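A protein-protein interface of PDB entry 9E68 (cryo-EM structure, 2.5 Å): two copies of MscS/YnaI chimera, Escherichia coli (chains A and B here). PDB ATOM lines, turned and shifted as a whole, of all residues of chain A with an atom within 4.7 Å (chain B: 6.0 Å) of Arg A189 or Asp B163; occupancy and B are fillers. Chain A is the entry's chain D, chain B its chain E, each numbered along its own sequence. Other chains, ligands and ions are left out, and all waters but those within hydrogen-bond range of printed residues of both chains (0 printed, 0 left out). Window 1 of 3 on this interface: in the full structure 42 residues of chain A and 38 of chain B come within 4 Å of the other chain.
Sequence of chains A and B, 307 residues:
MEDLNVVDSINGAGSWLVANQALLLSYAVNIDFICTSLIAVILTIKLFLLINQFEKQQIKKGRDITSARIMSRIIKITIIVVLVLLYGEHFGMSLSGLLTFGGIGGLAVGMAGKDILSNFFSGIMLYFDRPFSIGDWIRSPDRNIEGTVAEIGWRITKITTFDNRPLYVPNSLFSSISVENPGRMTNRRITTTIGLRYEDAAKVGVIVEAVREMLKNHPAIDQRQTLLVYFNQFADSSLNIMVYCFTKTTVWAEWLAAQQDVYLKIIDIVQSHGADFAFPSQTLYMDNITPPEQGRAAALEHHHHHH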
ATOM      1  N   ASN A 187       3.084   5.578   3.641  1.00  0.00           N
ATOM      2  CA  ASN A 187       3.163   6.854   2.945  1.00  0.00           C
ATOM      3  C   ASN A 187       3.286   6.602   1.451  1.00  0.00           C
ATOM      4  O   ASN A 187       3.644   5.506   1.013  1.00  0.00           O
ATOM      5  CB  ASN A 187       4.347   7.697   3.435  1.00  0.00           C
ATOM      6  CG  ASN A 187       4.146   8.225   4.839  1.00  0.00           C
ATOM      7  OD1 ASN A 187       4.659   7.662   5.805  1.00  0.00           O
ATOM      8  ND2 ASN A 187       3.399   9.315   4.961  1.00  0.00           N
ATOM      9  N   ARG A 188       2.981   7.633   0.672  1.00  0.00           N
ATOM     10  CA  ARG A 188       3.174   7.611  -0.769  1.00  0.00           C
ATOM     11  C   ARG A 188       4.288   8.576  -1.153  1.00  0.00           C
ATOM     12  O   ARG A 188       4.419   9.662  -0.583  1.00  0.00           O
ATOM     13  CB  ARG A 188       1.884   7.971  -1.507  1.00  0.00           C
ATOM     14  CG  ARG A 188       0.803   6.909  -1.406  1.00  0.00           C
ATOM     15  CD  ARG A 188      -0.153   6.981  -2.582  1.00  0.00           C
ATOM     16  NE  ARG A 188      -1.202   5.971  -2.503  1.00  0.00           N
ATOM     17  CZ  ARG A 188      -1.400   5.025  -3.409  1.00  0.00           C
ATOM     18  NH1 ARG A 188      -0.631   4.921  -4.480  1.00  0.00           N
ATOM     19  NH2 ARG A 188      -2.396   4.160  -3.238  1.00  0.00           N
ATOM     20  N   ARG A 189       5.090   8.169  -2.131  1.00  0.00           N
ATOM     21  CA  ARG A 189       6.321   8.862  -2.483  1.00  0.00           C
ATOM     22  C   ARG A 189       6.138   9.676  -3.756  1.00  0.00           C
ATOM     23  O   ARG A 189       5.441   9.252  -4.683  1.00  0.00           O
ATOM     24  CB  ARG A 189       7.466   7.864  -2.665  1.00  0.00           C
ATOM     25  CG  ARG A 189       8.842   8.495  -2.700  1.00  0.00           C
ATOM     26  CD  ARG A 189       9.917   7.433  -2.793  1.00  0.00           C
ATOM     27  NE  ARG A 189       9.737   6.575  -3.958  1.00  0.00           N
ATOM     28  CZ  ARG A 189      10.624   5.682  -4.371  1.00  0.00           C
ATOM     29  NH1 ARG A 189      11.766   5.495  -3.731  1.00  0.00           N
ATOM     30  NH2 ARG A 189      10.358   4.956  -5.453  1.00  0.00           N
ATOM     31  N   ILE A 190       6.770  10.847  -3.791  1.00  0.00           N
ATOM     32  CA  ILE A 190       6.807  11.702  -4.972  1.00  0.00           C
ATOM     33  C   ILE A 190       8.257  11.843  -5.409  1.00  0.00           C
ATOM     34  O   ILE A 190       9.107  12.276  -4.624  1.00  0.00           O
ATOM     35  CB  ILE A 190       6.186  13.083  -4.699  1.00  0.00           C
ATOM     36  CG1 ILE A 190       4.726  12.945  -4.273  1.00  0.00           C
ATOM     37  CG2 ILE A 190       6.309  13.973  -5.923  1.00  0.00           C
ATOM     38  CD1 ILE A 190       4.109  14.242  -3.814  1.00  0.00           C
ATOM     39  N   THR A 191       8.536  11.478  -6.658  1.00  0.00           N
ATOM     40  CA  THR A 191       9.873  11.596  -7.221  1.00  0.00           C
ATOM     41  C   THR A 191       9.775  12.170  -8.625  1.00  0.00           C
ATOM     42  O   THR A 191       8.899  11.779  -9.401  1.00  0.00           O
ATOM     43  CB  THR A 191      10.591  10.241  -7.264  1.00  0.00           C
ATOM     44  OG1 THR A 191       9.702   9.243  -7.780  1.00  0.00           O
ATOM     45  CG2 THR A 191      11.046   9.834  -5.872  1.00  0.00           C
ATOM     46  N   TYR A 244      12.664  14.286  -3.919  1.00  0.00           N
ATOM     47  CA  TYR A 244      12.365  13.071  -3.164  1.00  0.00           C
ATOM     48  C   TYR A 244      11.632  13.479  -1.895  1.00  0.00           C
ATOM     49  O   TYR A 244      12.219  14.129  -1.026  1.00  0.00           O
ATOM     50  CB  TYR A 244      13.650  12.312  -2.843  1.00  0.00           C
ATOM     51  CG  TYR A 244      13.462  10.855  -2.489  1.00  0.00           C
ATOM     52  CD1 TYR A 244      13.006  10.478  -1.234  1.00  0.00           C
ATOM     53  CD2 TYR A 244      13.758   9.857  -3.405  1.00  0.00           C
ATOM     54  CE1 TYR A 244      12.840   9.149  -0.906  1.00  0.00           C
ATOM     55  CE2 TYR A 244      13.595   8.525  -3.086  1.00  0.00           C
ATOM     56  CZ  TYR A 244      13.137   8.176  -1.836  1.00  0.00           C
ATOM     57  OH  TYR A 244      12.972   6.849  -1.513  1.00  0.00           O
ATOM     58  N   CYS A 245      10.359  13.105  -1.786  1.00  0.00           N
ATOM     59  CA  CYS A 245       9.547  13.467  -0.632  1.00  0.00           C
ATOM     60  C   CYS A 245       8.420  12.453  -0.479  1.00  0.00           C
ATOM     61  O   CYS A 245       8.210  11.591  -1.337  1.00  0.00           O
ATOM     62  CB  CYS A 245       9.003  14.892  -0.768  1.00  0.00           C
ATOM     63  SG  CYS A 245       7.954  15.157  -2.212  1.00  0.00           S
ATOM     64  N   PHE A 246       7.689  12.567   0.629  1.00  0.00           N
ATOM     65  CA  PHE A 246       6.591  11.667   0.949  1.00  0.00           C
ATOM     66  C   PHE A 246       5.361  12.466   1.352  1.00  0.00           C
ATOM     67  O   PHE A 246       5.466  13.565   1.904  1.00  0.00           O
ATOM     68  CB  PHE A 246       6.962  10.704   2.086  1.00  0.00           C
ATOM     69  CG  PHE A 246       7.866   9.583   1.666  1.00  0.00           C
ATOM     70  CD1 PHE A 246       7.341   8.392   1.197  1.00  0.00           C
ATOM     71  CD2 PHE A 246       9.241   9.717   1.748  1.00  0.00           C
ATOM     72  CE1 PHE A 246       8.169   7.358   0.814  1.00  0.00           C
ATOM     73  CE2 PHE A 246      10.074   8.685   1.366  1.00  0.00           C
ATOM     74  CZ  PHE A 246       9.537   7.505   0.898  1.00  0.00           C
ATOM     75  N   TRP A 255      -3.465  12.017  -3.153  1.00  0.00           N
ATOM     76  CA  TRP A 255      -2.047  11.882  -3.469  1.00  0.00           C
ATOM     77  C   TRP A 255      -1.748  12.446  -4.852  1.00  0.00           C
ATOM     78  O   TRP A 255      -0.782  13.196  -5.038  1.00  0.00           O
ATOM     79  CB  TRP A 255      -1.620  10.419  -3.383  1.00  0.00           C
ATOM     80  CG  TRP A 255      -0.293  10.162  -4.020  1.00  0.00           C
ATOM     81  CD1 TRP A 255       0.906  10.704  -3.662  1.00  0.00           C
ATOM     82  CD2 TRP A 255      -0.031   9.315  -5.144  1.00  0.00           C
ATOM     83  NE1 TRP A 255       1.900  10.239  -4.485  1.00  0.00           N
ATOM     84  CE2 TRP A 255       1.351   9.385  -5.405  1.00  0.00           C
ATOM     85  CE3 TRP A 255      -0.830   8.501  -5.950  1.00  0.00           C
ATOM     86  CZ2 TRP A 255       1.950   8.672  -6.439  1.00  0.00           C
ATOM     87  CZ3 TRP A 255      -0.232   7.795  -6.976  1.00  0.00           C
ATOM     88  CH2 TRP A 255       1.144   7.884  -7.211  1.00  0.00           C
ATOM     89  N   THR B 161      10.728  -1.556   2.164  1.00  0.00           N
ATOM     90  CA  THR B 161      11.280  -0.912   0.985  1.00  0.00           C
ATOM     91  C   THR B 161      11.382   0.597   1.202  1.00  0.00           C
ATOM     92  O   THR B 161      10.948   1.141   2.220  1.00  0.00           O
ATOM     93  CB  THR B 161      10.421  -1.211  -0.243  1.00  0.00           C
ATOM     94  OG1 THR B 161       9.144  -0.581  -0.099  1.00  0.00           O
ATOM     95  CG2 THR B 161      10.224  -2.708  -0.400  1.00  0.00           C
ATOM     96  N   PHE B 162      11.966   1.277   0.219  1.00  0.00           N
ATOM     97  CA  PHE B 162      12.110   2.725   0.283  1.00  0.00           C
ATOM     98  C   PHE B 162      10.833   3.460  -0.092  1.00  0.00           C
ATOM     99  O   PHE B 162      10.792   4.691   0.010  1.00  0.00           O
ATOM    100  CB  PHE B 162      13.263   3.178  -0.615  1.00  0.00           C
ATOM    101  CG  PHE B 162      14.619   2.864  -0.053  1.00  0.00           C
ATOM    102  CD1 PHE B 162      15.127   3.593   1.009  1.00  0.00           C
ATOM    103  CD2 PHE B 162      15.381   1.836  -0.577  1.00  0.00           C
ATOM    104  CE1 PHE B 162      16.372   3.307   1.532  1.00  0.00           C
ATOM    105  CE2 PHE B 162      16.627   1.545  -0.058  1.00  0.00           C
ATOM    106  CZ  PHE B 162      17.122   2.281   0.999  1.00  0.00           C
ATOM    107  N   ASP B 163       9.799   2.743  -0.523  1.00  0.00           N
ATOM    108  CA  ASP B 163       8.471   3.305  -0.716  1.00  0.00           C
ATOM    109  C   ASP B 163       7.600   3.161   0.524  1.00  0.00           C
ATOM    110  O   ASP B 163       6.392   3.405   0.449  1.00  0.00           O
ATOM    111  CB  ASP B 163       7.782   2.642  -1.910  1.00  0.00           C
ATOM    112  CG  ASP B 163       8.653   2.622  -3.147  1.00  0.00           C
ATOM    113  OD1 ASP B 163       8.124   2.334  -4.241  1.00  0.00           O
ATOM    114  OD2 ASP B 163       9.865   2.893  -3.024  1.00  0.00           O
ATOM    115  N   ASN B 164       8.190   2.763   1.654  1.00  0.00           N
ATOM    116  CA  ASN B 164       7.463   2.511   2.897  1.00  0.00           C
ATOM    117  C   ASN B 164       6.394   1.437   2.701  1.00  0.00           C
ATOM    118  O   ASN B 164       5.261   1.558   3.170  1.00  0.00           O
ATOM    119  CB  ASN B 164       6.857   3.800   3.456  1.00  0.00           C
ATOM    120  CG  ASN B 164       7.907   4.835   3.800  1.00  0.00           C
ATOM    121  OD1 ASN B 164       7.623   6.030   3.851  1.00  0.00           O
ATOM    122  ND2 ASN B 164       9.131   4.380   4.033  1.00  0.00           N
ATOM    123  N   ARG B 165       6.768   0.372   1.993  1.00  0.00           N
ATOM    124  CA  ARG B 165       5.906  -0.775   1.787  1.00  0.00           C
ATOM    125  C   ARG B 165       6.594  -2.043   2.281  1.00  0.00           C
ATOM    126  O   ARG B 165       7.782  -2.246   2.010  1.00  0.00           O
ATOM    127  CB  ARG B 165       5.543  -0.942   0.305  1.00  0.00           C
ATOM    128  CG  ARG B 165       5.129   0.342  -0.390  1.00  0.00           C
ATOM    129  CD  ARG B 165       4.863   0.093  -1.865  1.00  0.00           C
ATOM    130  NE  ARG B 165       4.105   1.172  -2.484  1.00  0.00           N
ATOM    131  CZ  ARG B 165       3.761   1.204  -3.764  1.00  0.00           C
ATOM    132  NH1 ARG B 165       4.093   0.228  -4.593  1.00  0.00           N
ATOM    133  NH2 ARG B 165       3.066   2.240  -4.224  1.00  0.00           N
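OD2 of Asp B163 lies within salt-bridge range of NH2 of Arg A189, at 3.2 Å. O of Phe B162 is in hydrogen-bond range of OH of Tyr A244, at 3.4 Å.
Arg A189 touches two residues of chain B. Asp B163 touches just these residues of chain A: Asn A187 (3.5 Å) and Arg A189 (3.2 Å). Printed residues of chain B within 4 Å of Phe A246: Phe B162 and Asn B164. Of the printed residues of chain A, Phe B162 touches Arg A189, Tyr A244 and Phe A246. Printed residues of chain B within 4 Å of Tyr A244: Phe B162. Of the printed residues of chain A, Asn B164 touches Asn A187 and Phe A246. The nearest printed residue of chain B that does not touch Arg A189 is Arg B165 (6.6 Å). The nearest printed residue of chain A that does not touch Asn B164 is Arg A188 (5.9 Å).
No position is printed for both chains.
Asp B163 touches Asn A187. Asn A187 touches Asn B164 (CB to OD1, 3.7 Å). Phe B162 touches Arg A189. Phe A246 touches Phe B162. Asn B164 touches Phe A246.
The guanidinium group (NH1) of Arg A189 is in hydrogen-bond range of the side-chain hydroxyl (OH) of Tyr A244 (2.9 Å). OG1 of Thr B161 lies close to N of Asp B163, at 3.4 Å.
Of the 5 printed residues of chain B, 3 touch a printed residue of chain A. Printed residues of chain B that touch a printed residue of chain A: Phe B162, Asp B163 and Asn B164. Hydrophobic or aromatic side chains of chain B that line the printed part of chain A: Phe B162. Of the 9 printed residues of chain A, 4 touch a printed residue of chain B. Printed residues of chain A that touch a printed residue of chain B: Asn A187, Arg A189, Tyr A244 and Phe A246. Hydrophobic or aromatic side chains of chain A within 4 Å of the printed part of chain B: Tyr A244 and Phe A246. Among the printed residues, 7 pairs touch across the chains.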
